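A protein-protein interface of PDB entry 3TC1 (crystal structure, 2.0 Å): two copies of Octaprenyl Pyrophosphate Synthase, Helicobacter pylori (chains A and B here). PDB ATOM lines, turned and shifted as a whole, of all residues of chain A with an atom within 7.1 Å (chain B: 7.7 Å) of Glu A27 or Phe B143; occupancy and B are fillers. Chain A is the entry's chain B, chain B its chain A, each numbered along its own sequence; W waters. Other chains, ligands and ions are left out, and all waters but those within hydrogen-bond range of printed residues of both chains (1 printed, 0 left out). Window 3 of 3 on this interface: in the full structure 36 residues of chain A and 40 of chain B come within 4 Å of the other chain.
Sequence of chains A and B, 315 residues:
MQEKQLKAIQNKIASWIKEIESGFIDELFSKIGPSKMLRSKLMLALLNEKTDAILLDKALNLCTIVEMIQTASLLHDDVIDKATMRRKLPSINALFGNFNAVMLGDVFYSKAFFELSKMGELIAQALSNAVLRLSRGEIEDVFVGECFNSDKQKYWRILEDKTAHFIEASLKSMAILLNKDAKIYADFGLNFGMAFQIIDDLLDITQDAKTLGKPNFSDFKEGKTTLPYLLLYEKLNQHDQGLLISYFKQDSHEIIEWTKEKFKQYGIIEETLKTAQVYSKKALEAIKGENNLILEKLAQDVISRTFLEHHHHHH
Ile A17 touches none of the printed residues of chain B.
Of the printed residues of chain B, Phe A24 touches Ile B139 (3.99 Å), Glu B140 (3.7 Å) and Phe B143 (3.4 Å).
Printed residues of chain B within 4 Å of Ile A25: Ile B139 (3.99 Å).
Of chain B, only Phe B143 (3.7 Å) comes within 4 Å of Glu A27.
Printed residues of chain B within 4 Å of Leu A28: Phe B143 (3.7 Å).
Ser A30 touches none of the printed residues of chain B.
Of the printed residues of chain B, Asn A100 touches Val B142 (3.8 Å) and Phe B143 (3.6 Å).
Of the printed residues of chain A, Val B142 touches Asn A100 (3.8 Å).
Of chain A, only Phe A24 (3.4 Å), Glu A27 (3.7 Å), Leu A28 (3.7 Å) and Asn A100 (3.6 Å) come within 4 Å of Phe B143.
The nearest printed residue of chain B that does not touch Glu A27 is Ile B139 (8.0 Å).
The nearest residue of chain A that does not touch Phe B143 is Phe A96 (4.5 Å).
The nearest printed residue of chain A that does not touch Ile B139 is Leu A28 (4.01 Å).
Water W1 bridges OE2 of Glu B140 (2.6 Å) and OG of Ser A22 (2.8 Å).
N of Ile A25 is in hydrogen-bond range of OG of Ser A22, at 3.2 Å.
The backbone carbonyl oxygen (O) of Glu A27 sits at hydrogen-bond distance from the side-chain hydroxyl (OG) of Ser A30, at 2.7 Å.
The backbone carbonyl oxygen (O) of Phe A96 is in hydrogen-bond range of the side-chain amide nitrogen (ND2) of Asn A100 (2.8 Å).
No position is printed for both chains.
Printed residues of chain A that touch a printed residue of chain B: Phe A24, Ile A25, Glu A27, Leu A28 and Asn A100.
Among the printed residues, no Asp or Glu carboxylate lies within 4 Å of a Lys or Arg side-chain nitrogen of the other chain.
Among the printed residues, merely in contact across the chains: Phe A24 with Ile B139 (3.99 Å), Phe A24 with Glu B140 (3.7 Å), Phe A24 with Phe B143 (3.4 Å), Ile A25 with Ile B139 (3.99 Å), Glu A27 with Phe B143 (3.7 Å), Leu A28 with Phe B143 (3.7 Å), Asn A100 with Val B142 (3.8 Å) and Asn A100 with Phe B143 (3.6 Å).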
ATOM      1  N   ILE A  17      11.148   2.700  12.258  1.00  0.00           N
ATOM      2  CA  ILE A  17      12.144   3.757  12.086  1.00  0.00           C
ATOM      3  C   ILE A  17      12.343   4.458  13.428  1.00  0.00           C
ATOM      4  O   ILE A  17      13.467   4.771  13.809  1.00  0.00           O
ATOM      5  CB  ILE A  17      11.708   4.799  11.020  1.00  0.00           C
ATOM      6  CG1 ILE A  17      11.795   4.179   9.628  1.00  0.00           C
ATOM      7  CG2 ILE A  17      12.603   6.043  11.087  1.00  0.00           C
ATOM      8  CD1 ILE A  17      13.189   3.736   9.240  1.00  0.00           C
ATOM      9  N   SER A  22      16.905   7.713  16.423  1.00  0.00           N
ATOM     10  CA  SER A  22      17.894   8.619  15.875  1.00  0.00           C
ATOM     11  C   SER A  22      17.184   9.789  15.208  1.00  0.00           C
ATOM     12  O   SER A  22      16.497   9.614  14.203  1.00  0.00           O
ATOM     13  CB  SER A  22      18.766   7.889  14.858  1.00  0.00           C
ATOM     14  OG  SER A  22      19.557   8.805  14.126  1.00  0.00           O
ATOM     15  N   GLY A  23      17.345  10.979  15.780  1.00  0.00           N
ATOM     16  CA  GLY A  23      16.716  12.161  15.222  1.00  0.00           C
ATOM     17  C   GLY A  23      17.182  12.416  13.801  1.00  0.00           C
ATOM     18  O   GLY A  23      16.426  12.917  12.970  1.00  0.00           O
ATOM     19  N   PHE A  24      18.432  12.065  13.519  1.00  0.00           N
ATOM     20  CA  PHE A  24      18.987  12.261  12.187  1.00  0.00           C
ATOM     21  C   PHE A  24      18.284  11.359  11.181  1.00  0.00           C
ATOM     22  O   PHE A  24      17.943  11.787  10.080  1.00  0.00           O
ATOM     23  CB  PHE A  24      20.488  11.964  12.185  1.00  0.00           C
ATOM     24  CG  PHE A  24      21.275  12.795  13.160  1.00  0.00           C
ATOM     25  CD1 PHE A  24      21.041  14.162  13.279  1.00  0.00           C
ATOM     26  CD2 PHE A  24      22.273  12.217  13.939  1.00  0.00           C
ATOM     27  CE1 PHE A  24      21.789  14.942  14.162  1.00  0.00           C
ATOM     28  CE2 PHE A  24      23.029  12.986  14.823  1.00  0.00           C
ATOM     29  CZ  PHE A  24      22.787  14.350  14.935  1.00  0.00           C
ATOM     30  N   ILE A  25      18.081  10.100  11.557  1.00  0.00           N
ATOM     31  CA  ILE A  25      17.402   9.170  10.673  1.00  0.00           C
ATOM     32  C   ILE A  25      15.945   9.596  10.507  1.00  0.00           C
ATOM     33  O   ILE A  25      15.382   9.470   9.418  1.00  0.00           O
ATOM     34  CB  ILE A  25      17.516   7.721  11.209  1.00  0.00           C
ATOM     35  CG1 ILE A  25      18.948   7.221  10.985  1.00  0.00           C
ATOM     36  CG2 ILE A  25      16.508   6.810  10.515  1.00  0.00           C
ATOM     37  CD1 ILE A  25      19.253   5.863  11.595  1.00  0.00           C
ATOM     38  N   ASP A  26      15.334  10.115  11.570  1.00  0.00           N
ATOM     39  CA  ASP A  26      13.948  10.570  11.474  1.00  0.00           C
ATOM     40  C   ASP A  26      13.854  11.643  10.396  1.00  0.00           C
ATOM     41  O   ASP A  26      12.880  11.700   9.639  1.00  0.00           O
ATOM     42  CB  ASP A  26      13.456  11.174  12.792  1.00  0.00           C
ATOM     43  CG  ASP A  26      13.314  10.149  13.900  1.00  0.00           C
ATOM     44  OD1 ASP A  26      13.145   8.945  13.603  1.00  0.00           O
ATOM     45  OD2 ASP A  26      13.349  10.562  15.077  1.00  0.00           O
ATOM     46  N   GLU A  27      14.875  12.495  10.334  1.00  0.00           N
ATOM     47  CA  GLU A  27      14.912  13.573   9.353  1.00  0.00           C
ATOM     48  C   GLU A  27      14.996  13.014   7.935  1.00  0.00           C
ATOM     49  O   GLU A  27      14.259  13.440   7.046  1.00  0.00           O
ATOM     50  CB  GLU A  27      16.111  14.484   9.622  1.00  0.00           C
ATOM     51  CG  GLU A  27      16.103  15.773   8.821  1.00  0.00           C
ATOM     52  CD  GLU A  27      17.374  16.576   9.009  1.00  0.00           C
ATOM     53  OE1 GLU A  27      17.793  16.763  10.172  1.00  0.00           O
ATOM     54  OE2 GLU A  27      17.950  17.024   7.994  1.00  0.00           O
ATOM     55  N   LEU A  28      15.898  12.061   7.724  1.00  0.00           N
ATOM     56  CA  LEU A  28      16.058  11.449   6.409  1.00  0.00           C
ATOM     57  C   LEU A  28      14.763  10.761   5.981  1.00  0.00           C
ATOM     58  O   LEU A  28      14.292  10.938   4.855  1.00  0.00           O
ATOM     59  CB  LEU A  28      17.193  10.423   6.435  1.00  0.00           C
ATOM     60  CG  LEU A  28      18.581  10.926   6.850  1.00  0.00           C
ATOM     61  CD1 LEU A  28      19.564   9.759   6.875  1.00  0.00           C
ATOM     62  CD2 LEU A  28      19.050  11.995   5.879  1.00  0.00           C
ATOM     63  N   PHE A  29      14.195   9.976   6.893  1.00  0.00           N
ATOM     64  CA  PHE A  29      12.958   9.249   6.625  1.00  0.00           C
ATOM     65  C   PHE A  29      11.787  10.151   6.223  1.00  0.00           C
ATOM     66  O   PHE A  29      10.963   9.766   5.390  1.00  0.00           O
ATOM     67  CB  PHE A  29      12.552   8.419   7.851  1.00  0.00           C
ATOM     68  CG  PHE A  29      11.291   7.619   7.652  1.00  0.00           C
ATOM     69  CD1 PHE A  29      11.230   6.621   6.681  1.00  0.00           C
ATOM     70  CD2 PHE A  29      10.161   7.874   8.423  1.00  0.00           C
ATOM     71  CE1 PHE A  29      10.056   5.889   6.479  1.00  0.00           C
ATOM     72  CE2 PHE A  29       8.980   7.146   8.231  1.00  0.00           C
ATOM     73  CZ  PHE A  29       8.929   6.154   7.257  1.00  0.00           C
ATOM     74  N   SER A  30      11.710  11.342   6.813  1.00  0.00           N
ATOM     75  CA  SER A  30      10.621  12.269   6.513  1.00  0.00           C
ATOM     76  C   SER A  30      10.613  12.755   5.066  1.00  0.00           C
ATOM     77  O   SER A  30       9.605  13.278   4.595  1.00  0.00           O
ATOM     78  CB  SER A  30      10.670  13.486   7.443  1.00  0.00           C
ATOM     79  OG  SER A  30      11.760  14.337   7.126  1.00  0.00           O
ATOM     80  N   LYS A  31      11.726  12.582   4.360  1.00  0.00           N
ATOM     81  CA  LYS A  31      11.802  13.032   2.975  1.00  0.00           C
ATOM     82  C   LYS A  31      11.480  11.970   1.942  1.00  0.00           C
ATOM     83  O   LYS A  31      11.515  12.236   0.739  1.00  0.00           O
ATOM     84  CB  LYS A  31      13.179  13.634   2.687  1.00  0.00           C
ATOM     85  CG  LYS A  31      13.365  15.005   3.311  1.00  0.00           C
ATOM     86  CD  LYS A  31      12.273  15.958   2.843  1.00  0.00           C
ATOM     87  CE  LYS A  31      12.397  17.318   3.507  1.00  0.00           C
ATOM     88  NZ  LYS A  31      12.284  17.219   4.988  1.00  0.00           N
ATOM     89  N   ILE A  32      11.175  10.763   2.410  1.00  0.00           N
ATOM     90  CA  ILE A  32      10.811   9.679   1.507  1.00  0.00           C
ATOM     91  C   ILE A  32       9.301   9.755   1.355  1.00  0.00           C
ATOM     92  O   ILE A  32       8.575   9.868   2.343  1.00  0.00           O
ATOM     93  CB  ILE A  32      11.194   8.306   2.082  1.00  0.00           C
ATOM     94  CG1 ILE A  32      12.696   8.271   2.369  1.00  0.00           C
ATOM     95  CG2 ILE A  32      10.820   7.203   1.091  1.00  0.00           C
ATOM     96  CD1 ILE A  32      13.172   6.983   3.001  1.00  0.00           C
ATOM     97  N   ILE A  92      16.630  11.189  -2.041  1.00  0.00           N
ATOM     98  CA  ILE A  92      17.320  11.304  -0.766  1.00  0.00           C
ATOM     99  C   ILE A  92      18.772  11.728  -0.981  1.00  0.00           C
ATOM    100  O   ILE A  92      19.317  12.512  -0.198  1.00  0.00           O
ATOM    101  CB  ILE A  92      17.270   9.970   0.024  1.00  0.00           C
ATOM    102  CG1 ILE A  92      15.841   9.714   0.505  1.00  0.00           C
ATOM    103  CG2 ILE A  92      18.213  10.024   1.226  1.00  0.00           C
ATOM    104  CD1 ILE A  92      15.300  10.807   1.430  1.00  0.00           C
ATOM    105  N   LEU A  95      18.968  15.485  -1.623  1.00  0.00           N
ATOM    106  CA  LEU A  95      18.729  16.307  -0.439  1.00  0.00           C
ATOM    107  C   LEU A  95      19.752  16.119   0.682  1.00  0.00           C
ATOM    108  O   LEU A  95      20.019  17.054   1.448  1.00  0.00           O
ATOM    109  CB  LEU A  95      17.329  16.017   0.122  1.00  0.00           C
ATOM    110  CG  LEU A  95      16.116  16.332  -0.760  1.00  0.00           C
ATOM    111  CD1 LEU A  95      14.861  15.746  -0.127  1.00  0.00           C
ATOM    112  CD2 LEU A  95      15.984  17.840  -0.938  1.00  0.00           C
ATOM    113  N   PHE A  96      20.334  14.924   0.778  1.00  0.00           N
ATOM    114  CA  PHE A  96      21.288  14.642   1.850  1.00  0.00           C
ATOM    115  C   PHE A  96      22.637  14.054   1.429  1.00  0.00           C
ATOM    116  O   PHE A  96      23.437  13.667   2.284  1.00  0.00           O
ATOM    117  CB  PHE A  96      20.622  13.712   2.867  1.00  0.00           C
ATOM    118  CG  PHE A  96      19.293  14.214   3.357  1.00  0.00           C
ATOM    119  CD1 PHE A  96      19.223  15.208   4.331  1.00  0.00           C
ATOM    120  CD2 PHE A  96      18.108  13.714   2.824  1.00  0.00           C
ATOM    121  CE1 PHE A  96      17.990  15.697   4.769  1.00  0.00           C
ATOM    122  CE2 PHE A  96      16.869  14.195   3.255  1.00  0.00           C
ATOM    123  CZ  PHE A  96      16.811  15.188   4.228  1.00  0.00           C
ATOM    124  N   ASN A 100      24.572   9.622   2.692  1.00  0.00           N
ATOM    125  CA  ASN A 100      23.396   9.437   3.534  1.00  0.00           C
ATOM    126  C   ASN A 100      22.364   8.525   2.884  1.00  0.00           C
ATOM    127  O   ASN A 100      21.764   7.685   3.558  1.00  0.00           O
ATOM    128  CB  ASN A 100      22.757  10.786   3.889  1.00  0.00           C
ATOM    129  CG  ASN A 100      23.462  11.483   5.046  1.00  0.00           C
ATOM    130  OD1 ASN A 100      23.726  10.876   6.088  1.00  0.00           O
ATOM    131  ND2 ASN A 100      23.756  12.766   4.870  1.00  0.00           N
ATOM    132  N   ARG B 136      23.724   3.469  11.733  1.00  0.00           N
ATOM    133  CA  ARG B 136      23.223   4.624  12.474  1.00  0.00           C
ATOM    134  C   ARG B 136      24.429   5.464  12.851  1.00  0.00           C
ATOM    135  O   ARG B 136      24.404   6.688  12.826  1.00  0.00           O
ATOM    136  CB  ARG B 136      22.500   4.183  13.741  1.00  0.00           C
ATOM    137  CG  ARG B 136      21.999   5.339  14.593  1.00  0.00           C
ATOM    138  CD  ARG B 136      21.228   4.848  15.803  1.00  0.00           C
ATOM    139  NE  ARG B 136      22.095   4.222  16.799  1.00  0.00           N
ATOM    140  CZ  ARG B 136      21.660   3.422  17.768  1.00  0.00           C
ATOM    141  NH1 ARG B 136      20.367   3.146  17.867  1.00  0.00           N
ATOM    142  NH2 ARG B 136      22.512   2.905  18.645  1.00  0.00           N
ATOM    143  N   GLY B 137      25.503   4.779  13.217  1.00  0.00           N
ATOM    144  CA  GLY B 137      26.738   5.470  13.582  1.00  0.00           C
ATOM    145  C   GLY B 137      27.307   6.321  12.474  1.00  0.00           C
ATOM    146  O   GLY B 137      27.707   7.456  12.665  1.00  0.00           O
ATOM    147  N   GLU B 138      27.302   5.763  11.279  1.00  0.00           N
ATOM    148  CA  GLU B 138      27.804   6.476  10.093  1.00  0.00           C
ATOM    149  C   GLU B 138      27.045   7.750   9.865  1.00  0.00           C
ATOM    150  O   GLU B 138      27.587   8.805   9.621  1.00  0.00           O
ATOM    151  CB  GLU B 138      27.697   5.582   8.839  1.00  0.00           C
ATOM    152  CG  GLU B 138      28.700   4.459   8.811  1.00  0.00           C
ATOM    153  CD  GLU B 138      30.124   4.949   8.782  1.00  0.00           C
ATOM    154  OE1 GLU B 138      30.370   5.858   7.954  1.00  0.00           O
ATOM    155  OE2 GLU B 138      30.971   4.418   9.559  1.00  0.00           O
ATOM    156  N   ILE B 139      25.746   7.634   9.956  1.00  0.00           N
ATOM    157  CA  ILE B 139      24.878   8.772   9.776  1.00  0.00           C
ATOM    158  C   ILE B 139      25.062   9.835  10.838  1.00  0.00           C
ATOM    159  O   ILE B 139      25.102  11.028  10.535  1.00  0.00           O
ATOM    160  CB  ILE B 139      23.400   8.299   9.684  1.00  0.00           C
ATOM    161  CG1 ILE B 139      23.236   7.488   8.393  1.00  0.00           C
ATOM    162  CG2 ILE B 139      22.443   9.530   9.693  1.00  0.00           C
ATOM    163  CD1 ILE B 139      21.857   6.790   8.290  1.00  0.00           C
ATOM    164  N   GLU B 140      25.205   9.403  12.078  1.00  0.00           N
ATOM    165  CA  GLU B 140      25.428  10.343  13.173  1.00  0.00           C
ATOM    166  C   GLU B 140      26.747  11.087  12.926  1.00  0.00           C
ATOM    167  O   GLU B 140      26.847  12.298  13.168  1.00  0.00           O
ATOM    168  CB  GLU B 140      25.509   9.611  14.529  1.00  0.00           C
ATOM    169  CG  GLU B 140      24.271   8.792  14.879  1.00  0.00           C
ATOM    170  CD  GLU B 140      24.446   7.915  16.117  1.00  0.00           C
ATOM    171  OE1 GLU B 140      25.449   7.177  16.192  1.00  0.00           O
ATOM    172  OE2 GLU B 140      23.570   7.952  17.009  1.00  0.00           O
ATOM    173  N   ASP B 141      27.745  10.355  12.439  1.00  0.00           N
ATOM    174  CA  ASP B 141      29.061  10.916  12.157  1.00  0.00           C
ATOM    175  C   ASP B 141      28.954  12.035  11.117  1.00  0.00           C
ATOM    176  O   ASP B 141      29.557  13.098  11.275  1.00  0.00           O
ATOM    177  CB  ASP B 141      29.989   9.797  11.658  1.00  0.00           C
ATOM    178  CG  ASP B 141      31.431   9.965  12.129  1.00  0.00           C
ATOM    179  OD1 ASP B 141      31.689  10.799  13.026  1.00  0.00           O
ATOM    180  OD2 ASP B 141      32.312   9.248  11.611  1.00  0.00           O
ATOM    181  N   VAL B 142      28.185  11.804  10.056  1.00  0.00           N
ATOM    182  CA  VAL B 142      28.025  12.823   9.025  1.00  0.00           C
ATOM    183  C   VAL B 142      27.301  14.060   9.550  1.00  0.00           C
ATOM    184  O   VAL B 142      27.785  15.178   9.376  1.00  0.00           O
ATOM    185  CB  VAL B 142      27.273  12.264   7.798  1.00  0.00           C
ATOM    186  CG1 VAL B 142      26.893  13.395   6.848  1.00  0.00           C
ATOM    187  CG2 VAL B 142      28.162  11.277   7.079  1.00  0.00           C
ATOM    188  N   PHE B 143      26.154  13.864  10.197  1.00  0.00           N
ATOM    189  CA  PHE B 143      25.379  14.980  10.741  1.00  0.00           C
ATOM    190  C   PHE B 143      26.123  15.770  11.816  1.00  0.00           C
ATOM    191  O   PHE B 143      26.092  17.002  11.814  1.00  0.00           O
ATOM    192  CB  PHE B 143      24.041  14.491  11.304  1.00  0.00           C
ATOM    193  CG  PHE B 143      22.966  14.332  10.260  1.00  0.00           C
ATOM    194  CD1 PHE B 143      23.019  13.293   9.332  1.00  0.00           C
ATOM    195  CD2 PHE B 143      21.911  15.239  10.192  1.00  0.00           C
ATOM    196  CE1 PHE B 143      22.033  13.159   8.348  1.00  0.00           C
ATOM    197  CE2 PHE B 143      20.919  15.116   9.215  1.00  0.00           C
ATOM    198  CZ  PHE B 143      20.981  14.072   8.291  1.00  0.00           C
ATOM    199  N   VAL B 144      26.773  15.072  12.741  1.00  0.00           N
ATOM    200  CA  VAL B 144      27.530  15.749  13.789  1.00  0.00           C
ATOM    201  C   VAL B 144      28.732  16.444  13.154  1.00  0.00           C
ATOM    202  O   VAL B 144      29.210  17.462  13.659  1.00  0.00           O
ATOM    203  CB  VAL B 144      28.026  14.757  14.870  1.00  0.00           C
ATOM    204  CG1 VAL B 144      28.997  15.454  15.822  1.00  0.00           C
ATOM    205  CG2 VAL B 144      26.836  14.212  15.654  1.00  0.00           C
ATOM    206  N   GLY B 145      29.201  15.896  12.035  1.00  0.00           N
ATOM    207  CA  GLY B 145      30.343  16.466  11.339  1.00  0.00           C
ATOM    208  C   GLY B 145      30.048  17.669  10.453  1.00  0.00           C
ATOM    209  O   GLY B 145      30.925  18.128   9.720  1.00  0.00           O
ATOM    210  N   GLU B 146      28.822  18.180  10.509  1.00  0.00           N
ATOM    211  CA  GLU B 146      28.447  19.344   9.703  1.00  0.00           C
ATOM    212  C   GLU B 146      29.054  20.612  10.305  1.00  0.00           C
ATOM    213  O   GLU B 146      29.168  21.636   9.637  1.00  0.00           O
ATOM    214  CB  GLU B 146      26.923  19.475   9.628  1.00  0.00           C
ATOM    215  CG  GLU B 146      26.202  18.336   8.900  1.00  0.00           C
ATOM    216  CD  GLU B 146      26.259  18.453   7.384  1.00  0.00           C
ATOM    217  OE1 GLU B 146      26.241  19.592   6.870  1.00  0.00           O
ATOM    218  OE2 GLU B 146      26.297  17.403   6.706  1.00  0.00           O
ATOM    219  N   CYS B 147      29.426  20.543  11.579  1.00  0.00           N
ATOM    220  CA  CYS B 147      30.058  21.677  12.233  1.00  0.00           C
ATOM    221  C   CYS B 147      30.952  21.186  13.363  1.00  0.00           C
ATOM    222  O   CYS B 147      30.804  20.061  13.849  1.00  0.00           O
ATOM    223  CB  CYS B 147      29.007  22.678  12.749  1.00  0.00           C
ATOM    224  SG  CYS B 147      28.161  22.239  14.281  1.00  0.00           S
ATOM    225  N   LYS B 154      28.614  13.054  22.246  1.00  0.00           N
ATOM    226  CA  LYS B 154      28.178  12.735  20.893  1.00  0.00           C
ATOM    227  C   LYS B 154      29.276  11.875  20.261  1.00  0.00           C
ATOM    228  O   LYS B 154      29.000  10.955  19.492  1.00  0.00           O
ATOM    229  CB  LYS B 154      27.964  14.018  20.076  1.00  0.00           C
ATOM    230  CG  LYS B 154      26.800  14.878  20.559  1.00  0.00           C
ATOM    231  CD  LYS B 154      26.559  16.082  19.643  1.00  0.00           C
ATOM    232  CE  LYS B 154      25.402  16.936  20.149  1.00  0.00           C
ATOM    233  NZ  LYS B 154      25.170  18.138  19.301  1.00  0.00           N
ATOM    234  N   ILE B 158      28.943   7.937  18.862  1.00  0.00           N
ATOM    235  CA  ILE B 158      29.374   7.591  17.513  1.00  0.00           C
ATOM    236  C   ILE B 158      30.389   6.447  17.519  1.00  0.00           C
ATOM    237  O   ILE B 158      30.301   5.529  16.701  1.00  0.00           O
ATOM    238  CB  ILE B 158      29.980   8.834  16.810  1.00  0.00           C
ATOM    239  CG1 ILE B 158      28.866   9.857  16.553  1.00  0.00           C
ATOM    240  CG2 ILE B 158      30.688   8.426  15.507  1.00  0.00           C
ATOM    241  CD1 ILE B 158      29.360  11.245  16.172  1.00  0.00           C
ATOM    242  N   GLY B 223      35.844  16.694   8.883  1.00  0.00           N
ATOM    243  CA  GLY B 223      34.765  17.159   9.732  1.00  0.00           C
ATOM    244  C   GLY B 223      34.580  16.345  10.997  1.00  0.00           C
ATOM    245  O   GLY B 223      33.606  16.542  11.724  1.00  0.00           O
ATOM    246  N   LYS B 249      37.426  21.271   8.886  1.00  0.00           N
ATOM    247  CA  LYS B 249      37.242  20.861   7.492  1.00  0.00           C
ATOM    248  C   LYS B 249      38.178  21.512   6.478  1.00  0.00           C
ATOM    249  O   LYS B 249      37.890  21.515   5.281  1.00  0.00           O
ATOM    250  CB  LYS B 249      35.784  21.080   7.051  1.00  0.00           C
ATOM    251  CG  LYS B 249      34.831  19.982   7.514  1.00  0.00           C
ATOM    252  CD  LYS B 249      33.438  20.099   6.881  1.00  0.00           C
ATOM    253  CE  LYS B 249      32.567  18.906   7.287  1.00  0.00           C
ATOM    254  NZ  LYS B 249      31.199  18.903   6.686  1.00  0.00           N
HETATM  255  O   HOH W   1      21.547   9.244  16.088  1.00  0.00           O
